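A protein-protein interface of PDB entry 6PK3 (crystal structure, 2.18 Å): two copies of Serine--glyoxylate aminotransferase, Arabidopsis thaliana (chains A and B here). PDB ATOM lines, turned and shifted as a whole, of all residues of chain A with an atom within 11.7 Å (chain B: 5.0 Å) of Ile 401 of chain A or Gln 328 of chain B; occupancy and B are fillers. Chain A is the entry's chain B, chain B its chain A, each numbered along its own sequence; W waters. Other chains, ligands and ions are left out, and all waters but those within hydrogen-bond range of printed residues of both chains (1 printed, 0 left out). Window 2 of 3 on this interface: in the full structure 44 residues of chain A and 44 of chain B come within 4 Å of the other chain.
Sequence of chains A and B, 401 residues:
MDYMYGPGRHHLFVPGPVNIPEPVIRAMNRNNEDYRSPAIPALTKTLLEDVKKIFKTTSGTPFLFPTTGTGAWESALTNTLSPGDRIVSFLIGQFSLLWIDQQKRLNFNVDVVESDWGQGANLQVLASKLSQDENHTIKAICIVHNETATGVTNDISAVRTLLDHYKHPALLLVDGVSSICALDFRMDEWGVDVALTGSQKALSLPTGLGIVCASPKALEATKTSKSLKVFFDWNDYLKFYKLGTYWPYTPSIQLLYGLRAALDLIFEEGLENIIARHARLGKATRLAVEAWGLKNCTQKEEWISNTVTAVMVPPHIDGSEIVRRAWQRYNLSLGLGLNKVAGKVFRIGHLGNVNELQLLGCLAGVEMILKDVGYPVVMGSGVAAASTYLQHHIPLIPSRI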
ATOM      1  N   GLU A 268     -22.400  13.468 -42.053  1.00  0.00           N
ATOM      2  CA  GLU A 268     -23.586  13.685 -41.230  1.00  0.00           C
ATOM      3  C   GLU A 268     -23.204  14.203 -39.849  1.00  0.00           C
ATOM      4  O   GLU A 268     -23.780  15.180 -39.359  1.00  0.00           O
ATOM      5  CB  GLU A 268     -24.396  12.396 -41.114  1.00  0.00           C
ATOM      6  CG  GLU A 268     -25.899  12.623 -41.206  1.00  0.00           C
ATOM      7  CD  GLU A 268     -26.702  11.534 -40.523  1.00  0.00           C
ATOM      8  OE1 GLU A 268     -26.539  10.350 -40.889  1.00  0.00           O
ATOM      9  OE2 GLU A 268     -27.492  11.863 -39.612  1.00  0.00           O
ATOM     10  N   GLU A 269     -22.235  13.552 -39.199  1.00  0.00           N
ATOM     11  CA  GLU A 269     -21.760  14.048 -37.913  1.00  0.00           C
ATOM     12  C   GLU A 269     -21.051  15.387 -38.072  1.00  0.00           C
ATOM     13  O   GLU A 269     -21.161  16.264 -37.205  1.00  0.00           O
ATOM     14  CB  GLU A 269     -20.828  13.023 -37.265  1.00  0.00           C
ATOM     15  CG  GLU A 269     -20.279  13.461 -35.917  1.00  0.00           C
ATOM     16  CD  GLU A 269     -19.452  12.392 -35.236  1.00  0.00           C
ATOM     17  OE1 GLU A 269     -19.270  11.303 -35.823  1.00  0.00           O
ATOM     18  OE2 GLU A 269     -18.985  12.644 -34.104  1.00  0.00           O
ATOM     19  N   ARG A 280     -12.094  15.337 -27.159  1.00  0.00           N
ATOM     20  CA  ARG A 280     -12.704  14.990 -25.877  1.00  0.00           C
ATOM     21  C   ARG A 280     -12.199  13.644 -25.373  1.00  0.00           C
ATOM     22  O   ARG A 280     -11.869  13.496 -24.190  1.00  0.00           O
ATOM     23  CB  ARG A 280     -14.228  14.956 -26.004  1.00  0.00           C
ATOM     24  CG  ARG A 280     -14.883  16.308 -26.093  1.00  0.00           C
ATOM     25  CD  ARG A 280     -16.375  16.211 -25.796  1.00  0.00           C
ATOM     26  NE  ARG A 280     -17.042  15.210 -26.626  1.00  0.00           N
ATOM     27  CZ  ARG A 280     -17.481  15.429 -27.862  1.00  0.00           C
ATOM     28  NH1 ARG A 280     -17.325  16.616 -28.433  1.00  0.00           N
ATOM     29  NH2 ARG A 280     -18.078  14.453 -28.532  1.00  0.00           N
ATOM     30  N   ASN A 355     -17.793   6.327 -28.856  1.00  0.00           N
ATOM     31  CA  ASN A 355     -18.390   7.382 -28.045  1.00  0.00           C
ATOM     32  C   ASN A 355     -17.863   7.316 -26.615  1.00  0.00           C
ATOM     33  O   ASN A 355     -17.078   6.437 -26.247  1.00  0.00           O
ATOM     34  CB  ASN A 355     -19.921   7.308 -28.080  1.00  0.00           C
ATOM     35  CG  ASN A 355     -20.469   5.978 -27.591  1.00  0.00           C
ATOM     36  OD1 ASN A 355     -19.958   5.383 -26.641  1.00  0.00           O
ATOM     37  ND2 ASN A 355     -21.525   5.508 -28.243  1.00  0.00           N
ATOM     38  N   GLU A 356     -18.317   8.270 -25.799  1.00  0.00           N
ATOM     39  CA  GLU A 356     -17.706   8.489 -24.494  1.00  0.00           C
ATOM     40  C   GLU A 356     -17.980   7.338 -23.534  1.00  0.00           C
ATOM     41  O   GLU A 356     -17.107   6.968 -22.741  1.00  0.00           O
ATOM     42  CB  GLU A 356     -18.202   9.810 -23.904  1.00  0.00           C
ATOM     43  CG  GLU A 356     -17.667  11.046 -24.619  1.00  0.00           C
ATOM     44  CD  GLU A 356     -18.403  11.348 -25.917  1.00  0.00           C
ATOM     45  OE1 GLU A 356     -19.286  10.552 -26.301  1.00  0.00           O
ATOM     46  OE2 GLU A 356     -18.102  12.383 -26.549  1.00  0.00           O
ATOM     47  N   LEU A 357     -19.181   6.758 -23.578  1.00  0.00           N
ATOM     48  CA  LEU A 357     -19.473   5.663 -22.657  1.00  0.00           C
ATOM     49  C   LEU A 357     -18.664   4.417 -22.994  1.00  0.00           C
ATOM     50  O   LEU A 357     -18.321   3.642 -22.094  1.00  0.00           O
ATOM     51  CB  LEU A 357     -20.965   5.340 -22.656  1.00  0.00           C
ATOM     52  CG  LEU A 357     -21.933   6.407 -22.139  1.00  0.00           C
ATOM     53  CD1 LEU A 357     -23.205   5.736 -21.600  1.00  0.00           C
ATOM     54  CD2 LEU A 357     -21.322   7.300 -21.094  1.00  0.00           C
ATOM     55  N   LEU A 390     -15.922  15.196 -19.075  1.00  0.00           N
ATOM     56  CA  LEU A 390     -16.836  14.924 -20.180  1.00  0.00           C
ATOM     57  C   LEU A 390     -18.247  15.430 -19.901  1.00  0.00           C
ATOM     58  O   LEU A 390     -18.942  15.857 -20.831  1.00  0.00           O
ATOM     59  CB  LEU A 390     -16.864  13.427 -20.474  1.00  0.00           C
ATOM     60  CG  LEU A 390     -15.576  12.839 -21.047  1.00  0.00           C
ATOM     61  CD1 LEU A 390     -15.626  11.320 -20.997  1.00  0.00           C
ATOM     62  CD2 LEU A 390     -15.352  13.317 -22.469  1.00  0.00           C
ATOM     63  N   GLN A 391     -18.696  15.385 -18.643  1.00  0.00           N
ATOM     64  CA  GLN A 391     -20.024  15.896 -18.316  1.00  0.00           C
ATOM     65  C   GLN A 391     -20.175  17.365 -18.683  1.00  0.00           C
ATOM     66  O   GLN A 391     -21.305  17.847 -18.830  1.00  0.00           O
ATOM     67  CB  GLN A 391     -20.312  15.705 -16.825  1.00  0.00           C
ATOM     68  CG  GLN A 391     -21.730  16.095 -16.410  1.00  0.00           C
ATOM     69  CD  GLN A 391     -21.848  17.540 -15.941  1.00  0.00           C
ATOM     70  OE1 GLN A 391     -20.847  18.212 -15.699  1.00  0.00           O
ATOM     71  NE2 GLN A 391     -23.081  18.020 -15.809  1.00  0.00           N
ATOM     72  N   HIS A 393     -18.582  18.754 -21.495  1.00  0.00           N
ATOM     73  CA  HIS A 393     -18.282  19.001 -22.897  1.00  0.00           C
ATOM     74  C   HIS A 393     -19.025  18.121 -23.889  1.00  0.00           C
ATOM     75  O   HIS A 393     -19.054  18.466 -25.075  1.00  0.00           O
ATOM     76  CB  HIS A 393     -16.774  18.837 -23.149  1.00  0.00           C
ATOM     77  CG  HIS A 393     -15.949  19.931 -22.554  1.00  0.00           C
ATOM     78  ND1 HIS A 393     -15.407  19.852 -21.290  1.00  0.00           N
ATOM     79  CD2 HIS A 393     -15.592  21.142 -23.041  1.00  0.00           C
ATOM     80  CE1 HIS A 393     -14.743  20.964 -21.028  1.00  0.00           C
ATOM     81  NE2 HIS A 393     -14.841  21.763 -22.075  1.00  0.00           N
ATOM     82  N   ILE A 394     -19.615  17.009 -23.464  1.00  0.00           N
ATOM     83  CA  ILE A 394     -20.320  16.170 -24.442  1.00  0.00           C
ATOM     84  C   ILE A 394     -21.457  16.974 -25.059  1.00  0.00           C
ATOM     85  O   ILE A 394     -22.305  17.512 -24.323  1.00  0.00           O
ATOM     86  CB  ILE A 394     -20.857  14.889 -23.782  1.00  0.00           C
ATOM     87  CG1 ILE A 394     -19.705  13.963 -23.400  1.00  0.00           C
ATOM     88  CG2 ILE A 394     -21.831  14.180 -24.731  1.00  0.00           C
ATOM     89  CD1 ILE A 394     -20.117  12.812 -22.505  1.00  0.00           C
ATOM     90  N   PRO A 395     -21.534  17.099 -26.381  1.00  0.00           N
ATOM     91  CA  PRO A 395     -22.666  17.803 -26.989  1.00  0.00           C
ATOM     92  C   PRO A 395     -23.890  16.907 -27.099  1.00  0.00           C
ATOM     93  O   PRO A 395     -23.802  15.678 -27.115  1.00  0.00           O
ATOM     94  CB  PRO A 395     -22.139  18.187 -28.374  1.00  0.00           C
ATOM     95  CG  PRO A 395     -21.167  17.098 -28.705  1.00  0.00           C
ATOM     96  CD  PRO A 395     -20.552  16.661 -27.392  1.00  0.00           C
ATOM     97  N   LEU A 396     -25.050  17.552 -27.163  1.00  0.00           N
ATOM     98  CA  LEU A 396     -26.282  16.828 -27.432  1.00  0.00           C
ATOM     99  C   LEU A 396     -26.276  16.299 -28.863  1.00  0.00           C
ATOM    100  O   LEU A 396     -25.734  16.925 -29.779  1.00  0.00           O
ATOM    101  CB  LEU A 396     -27.494  17.731 -27.205  1.00  0.00           C
ATOM    102  CG  LEU A 396     -27.766  18.123 -25.750  1.00  0.00           C
ATOM    103  CD1 LEU A 396     -28.714  19.303 -25.689  1.00  0.00           C
ATOM    104  CD2 LEU A 396     -28.335  16.950 -24.973  1.00  0.00           C
ATOM    105  N   ILE A 397     -26.876  15.129 -29.050  1.00  0.00           N
ATOM    106  CA  ILE A 397     -26.921  14.487 -30.364  1.00  0.00           C
ATOM    107  C   ILE A 397     -27.902  15.255 -31.245  1.00  0.00           C
ATOM    108  O   ILE A 397     -29.111  15.252 -30.969  1.00  0.00           O
ATOM    109  CB  ILE A 397     -27.303  13.003 -30.240  1.00  0.00           C
ATOM    110  CG1 ILE A 397     -26.246  12.266 -29.412  1.00  0.00           C
ATOM    111  CG2 ILE A 397     -27.440  12.370 -31.616  1.00  0.00           C
ATOM    112  CD1 ILE A 397     -26.602  10.832 -29.081  1.00  0.00           C
ATOM    113  N   PRO A 398     -27.434  15.924 -32.309  1.00  0.00           N
ATOM    114  CA  PRO A 398     -28.352  16.772 -33.092  1.00  0.00           C
ATOM    115  C   PRO A 398     -29.534  16.022 -33.684  1.00  0.00           C
ATOM    116  O   PRO A 398     -30.633  16.584 -33.778  1.00  0.00           O
ATOM    117  CB  PRO A 398     -27.445  17.347 -34.192  1.00  0.00           C
ATOM    118  CG  PRO A 398     -26.061  17.232 -33.659  1.00  0.00           C
ATOM    119  CD  PRO A 398     -26.050  16.003 -32.810  1.00  0.00           C
ATOM    120  N   SER A 399     -29.339  14.767 -34.099  1.00  0.00           N
ATOM    121  CA  SER A 399     -30.432  14.001 -34.688  1.00  0.00           C
ATOM    122  C   SER A 399     -31.586  13.809 -33.713  1.00  0.00           C
ATOM    123  O   SER A 399     -32.708  13.517 -34.140  1.00  0.00           O
ATOM    124  CB  SER A 399     -29.924  12.635 -35.155  1.00  0.00           C
ATOM    125  OG  SER A 399     -29.479  11.861 -34.055  1.00  0.00           O
ATOM    126  N   ARG A 400     -31.333  13.969 -32.414  1.00  0.00           N
ATOM    127  CA  ARG A 400     -32.330  13.759 -31.372  1.00  0.00           C
ATOM    128  C   ARG A 400     -32.778  15.077 -30.751  1.00  0.00           C
ATOM    129  O   ARG A 400     -33.356  15.085 -29.660  1.00  0.00           O
ATOM    130  CB  ARG A 400     -31.759  12.799 -30.325  1.00  0.00           C
ATOM    131  CG  ARG A 400     -31.066  11.611 -30.995  1.00  0.00           C
ATOM    132  CD  ARG A 400     -30.422  10.607 -30.053  1.00  0.00           C
ATOM    133  NE  ARG A 400     -29.847   9.510 -30.834  1.00  0.00           N
ATOM    134  CZ  ARG A 400     -29.291   8.415 -30.326  1.00  0.00           C
ATOM    135  NH1 ARG A 400     -29.222   8.238 -29.012  1.00  0.00           N
ATOM    136  NH2 ARG A 400     -28.803   7.490 -31.143  1.00  0.00           N
ATOM    137  N   ILE A 401     -32.549  16.185 -31.457  1.00  0.00           N
ATOM    138  CA  ILE A 401     -32.857  17.536 -30.994  1.00  0.00           C
ATOM    139  C   ILE A 401     -32.167  17.799 -29.661  1.00  0.00           C
ATOM    140  O   ILE A 401     -31.202  18.562 -29.609  1.00  0.00           O
ATOM    141  CB  ILE A 401     -34.377  17.764 -30.900  1.00  0.00           C
ATOM    142  CG1 ILE A 401     -35.037  17.393 -32.232  1.00  0.00           C
ATOM    143  CG2 ILE A 401     -34.675  19.220 -30.553  1.00  0.00           C
ATOM    144  CD1 ILE A 401     -36.495  17.818 -32.354  1.00  0.00           C
ATOM    145  OXT ILE A 401     -32.539  17.258 -28.619  1.00  0.00           O
ATOM    146  N   ARG B 324     -34.642  10.274 -20.740  1.00  0.00           N
ATOM    147  CA  ARG B 324     -34.607  11.138 -21.913  1.00  0.00           C
ATOM    148  C   ARG B 324     -33.203  11.676 -22.164  1.00  0.00           C
ATOM    149  O   ARG B 324     -32.736  11.698 -23.310  1.00  0.00           O
ATOM    150  CB  ARG B 324     -35.604  12.282 -21.726  1.00  0.00           C
ATOM    151  CG  ARG B 324     -35.809  13.170 -22.941  1.00  0.00           C
ATOM    152  CD  ARG B 324     -36.926  14.204 -22.696  1.00  0.00           C
ATOM    153  NE  ARG B 324     -38.064  13.628 -21.971  1.00  0.00           N
ATOM    154  CZ  ARG B 324     -38.417  13.936 -20.721  1.00  0.00           C
ATOM    155  NH1 ARG B 324     -37.744  14.845 -20.022  1.00  0.00           N
ATOM    156  NH2 ARG B 324     -39.464  13.338 -20.167  1.00  0.00           N
ATOM    157  N   ARG B 325     -32.512  12.107 -21.105  1.00  0.00           N
ATOM    158  CA  ARG B 325     -31.171  12.659 -21.270  1.00  0.00           C
ATOM    159  C   ARG B 325     -30.175  11.583 -21.681  1.00  0.00           C
ATOM    160  O   ARG B 325     -29.257  11.848 -22.466  1.00  0.00           O
ATOM    161  CB  ARG B 325     -30.724  13.345 -19.980  1.00  0.00           C
ATOM    162  CG  ARG B 325     -31.381  14.697 -19.763  1.00  0.00           C
ATOM    163  CD  ARG B 325     -31.084  15.267 -18.383  1.00  0.00           C
ATOM    164  NE  ARG B 325     -31.746  16.554 -18.173  1.00  0.00           N
ATOM    165  CZ  ARG B 325     -31.194  17.740 -18.421  1.00  0.00           C
ATOM    166  NH1 ARG B 325     -29.954  17.828 -18.891  1.00  0.00           N
ATOM    167  NH2 ARG B 325     -31.889  18.846 -18.197  1.00  0.00           N
ATOM    168  N   ALA B 326     -30.334  10.364 -21.160  1.00  0.00           N
ATOM    169  CA  ALA B 326     -29.475   9.266 -21.590  1.00  0.00           C
ATOM    170  C   ALA B 326     -29.537   9.084 -23.102  1.00  0.00           C
ATOM    171  O   ALA B 326     -28.509   8.878 -23.757  1.00  0.00           O
ATOM    172  CB  ALA B 326     -29.879   7.975 -20.880  1.00  0.00           C
ATOM    173  N   TRP B 327     -30.739   9.174 -23.674  1.00  0.00           N
ATOM    174  CA  TRP B 327     -30.899   8.972 -25.108  1.00  0.00           C
ATOM    175  C   TRP B 327     -30.352  10.150 -25.902  1.00  0.00           C
ATOM    176  O   TRP B 327     -29.647   9.961 -26.899  1.00  0.00           O
ATOM    177  CB  TRP B 327     -32.376   8.746 -25.429  1.00  0.00           C
ATOM    178  CG  TRP B 327     -32.704   8.805 -26.885  1.00  0.00           C
ATOM    179  CD1 TRP B 327     -33.219   9.868 -27.565  1.00  0.00           C
ATOM    180  CD2 TRP B 327     -32.542   7.754 -27.844  1.00  0.00           C
ATOM    181  NE1 TRP B 327     -33.393   9.544 -28.887  1.00  0.00           N
ATOM    182  CE2 TRP B 327     -32.981   8.253 -29.086  1.00  0.00           C
ATOM    183  CE3 TRP B 327     -32.070   6.441 -27.774  1.00  0.00           C
ATOM    184  CZ2 TRP B 327     -32.961   7.485 -30.249  1.00  0.00           C
ATOM    185  CZ3 TRP B 327     -32.048   5.679 -28.930  1.00  0.00           C
ATOM    186  CH2 TRP B 327     -32.492   6.204 -30.149  1.00  0.00           C
ATOM    187  N   GLN B 328     -30.656  11.373 -25.469  1.00  0.00           N
ATOM    188  CA  GLN B 328     -30.335  12.548 -26.267  1.00  0.00           C
ATOM    189  C   GLN B 328     -28.856  12.904 -26.223  1.00  0.00           C
ATOM    190  O   GLN B 328     -28.329  13.438 -27.204  1.00  0.00           O
ATOM    191  CB  GLN B 328     -31.162  13.744 -25.790  1.00  0.00           C
ATOM    192  CG  GLN B 328     -32.603  13.727 -26.258  1.00  0.00           C
ATOM    193  CD  GLN B 328     -33.422  14.857 -25.660  1.00  0.00           C
ATOM    194  OE1 GLN B 328     -33.136  15.332 -24.561  1.00  0.00           O
ATOM    195  NE2 GLN B 328     -34.445  15.294 -26.387  1.00  0.00           N
ATOM    196  N   ARG B 329     -28.174  12.629 -25.113  1.00  0.00           N
ATOM    197  CA  ARG B 329     -26.807  13.097 -24.931  1.00  0.00           C
ATOM    198  C   ARG B 329     -25.767  11.991 -24.871  1.00  0.00           C
ATOM    199  O   ARG B 329     -24.634  12.211 -25.301  1.00  0.00           O
ATOM    200  CB  ARG B 329     -26.696  13.931 -23.647  1.00  0.00           C
ATOM    201  CG  ARG B 329     -25.349  14.617 -23.501  1.00  0.00           C
ATOM    202  CD  ARG B 329     -25.304  15.565 -22.316  1.00  0.00           C
ATOM    203  NE  ARG B 329     -24.140  16.442 -22.398  1.00  0.00           N
ATOM    204  CZ  ARG B 329     -23.582  17.062 -21.363  1.00  0.00           C
ATOM    205  NH1 ARG B 329     -24.071  16.904 -20.141  1.00  0.00           N
ATOM    206  NH2 ARG B 329     -22.527  17.842 -21.551  1.00  0.00           N
ATOM    207  N   TYR B 330     -26.111  10.815 -24.346  1.00  0.00           N
ATOM    208  CA  TYR B 330     -25.128   9.776 -24.080  1.00  0.00           C
ATOM    209  C   TYR B 330     -25.305   8.534 -24.942  1.00  0.00           C
ATOM    210  O   TYR B 330     -24.544   7.574 -24.778  1.00  0.00           O
ATOM    211  CB  TYR B 330     -25.173   9.392 -22.594  1.00  0.00           C
ATOM    212  CG  TYR B 330     -24.876  10.557 -21.677  1.00  0.00           C
ATOM    213  CD1 TYR B 330     -23.569  10.948 -21.423  1.00  0.00           C
ATOM    214  CD2 TYR B 330     -25.901  11.278 -21.082  1.00  0.00           C
ATOM    215  CE1 TYR B 330     -23.290  12.020 -20.594  1.00  0.00           C
ATOM    216  CE2 TYR B 330     -25.635  12.353 -20.249  1.00  0.00           C
ATOM    217  CZ  TYR B 330     -24.324  12.719 -20.009  1.00  0.00           C
ATOM    218  OH  TYR B 330     -24.049  13.789 -19.184  1.00  0.00           O
HETATM  219  O   HOH W   1     -21.694   7.815 -25.094  1.00  0.00           O
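The backbone carbonyl oxygen (O) of Trp 327 of chain B lies within hydrogen-bond range of the guanidinium group (NH1) of Arg 400 of chain A (2.8 Å). O of Gln 328 of chain B lies within hydrogen-bond range of N of Ile 397 of chain A. The side-chain amide nitrogen of Gln 328 of chain B is in hydrogen-bond range of the backbone carbonyl oxygen of Arg 400 of chain A (3.5 Å). The backbone carbonyl oxygen (O) of Gln 391 of chain A is in hydrogen-bond range of the guanidinium group (NH2) of Arg 329 of chain B, at 3.0 Å. The backbone carbonyl oxygen (O) of Ile 394 of chain A is in hydrogen-bond range of the guanidinium group (NH2) of Arg 329 of chain B.
The side-chain hydroxyl (OH) of Tyr 330 of chain B is in hydrogen-bond range of the guanidinium group (NH1) of Arg 329 of chain B (3.3 Å). The backbone NH (N) of Leu 357 of chain A lies close to the side-chain amide oxygen (OD1) of Asn 355 of chain A (3.4 Å).
Among the printed residues, merely in contact across the chains: Ile 401 of chain A with Gln 328 of chain B (3.5 Å), Leu 396 of chain A with Arg 329 of chain B (3.7 Å), Ile 394 of chain A with Tyr 330 of chain B (3.8 Å), Ile 397 of chain A with Trp 327 of chain B (3.8 Å), Leu 357 of chain A with Tyr 330 of chain B (3.9 Å) and Leu 396 of chain A with Gln 328 of chain B (3.9 Å).
Of the printed residues of chain B, Leu 357 of chain A touches Tyr 330. His 393 of chain A touches none of the printed residues of chain B. Of the printed residues of chain B, Ile 394 of chain A touches Arg 329 (2.8 Å) and Tyr 330 (3.8 Å). Printed residues of chain B within 4 Å of Arg 400 of chain A: Trp 327 (2.8 Å) and Gln 328 (3.5 Å). Ile 401 of chain A touches just one residue of chain B: Gln 328. No residue of chain A comes within 4 Å of Arg 325 of chain B. No residue of chain A comes within 4 Å of Ala 326 of chain B. Of chain A, only Leu 396 (3.9 Å), Ile 397 (2.9 Å), Arg 400 (3.5 Å) and Ile 401 (3.5 Å) come within 4 Å of Gln 328 of chain B. Of the printed residues of chain A, Tyr 330 of chain B touches Leu 357 and Ile 394. The nearest printed residue of chain B that does not touch Ile 401 of chain A is Trp 327 of chain B (7.2 Å). The nearest printed residue of chain A that does not touch Arg 329 of chain B is Pro 395 of chain A (4.0004 Å).
Of the 7 printed residues of chain B, 4 touch a printed residue of chain A. Printed residues of chain B that touch a printed residue of chain A: Trp 327, Gln 328, Arg 329 and Tyr 330. Of the 17 printed residues of chain A, 7 touch a printed residue of chain B. Printed residues of chain A that touch a printed residue of chain B: Leu 357, Gln 391, Ile 394, Leu 396, Ile 397, Arg 400 and Ile 401. Hydrophobic or aromatic side chains of chain A that line the printed part of chain B: Leu 357, Ile 394, Leu 396 and Ile 397. Among the printed residues, 11 pairs touch across the chains.
No position is printed for both chains. Of the 11 pairs that touch across the chains among the printed residues, none has its exchanged pair printed and touching as well.
Water W1 lies within hydrogen-bond range of the backbone carbonyl oxygen of Tyr 330 of chain B (2.9 Å), the backbone NH of Leu 357 of chain A (3.1 Å), the side-chain amide oxygen of Asn 355 of chain A (3.4 Å) and the backbone NH of Glu 356 of chain A (3.5 Å).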
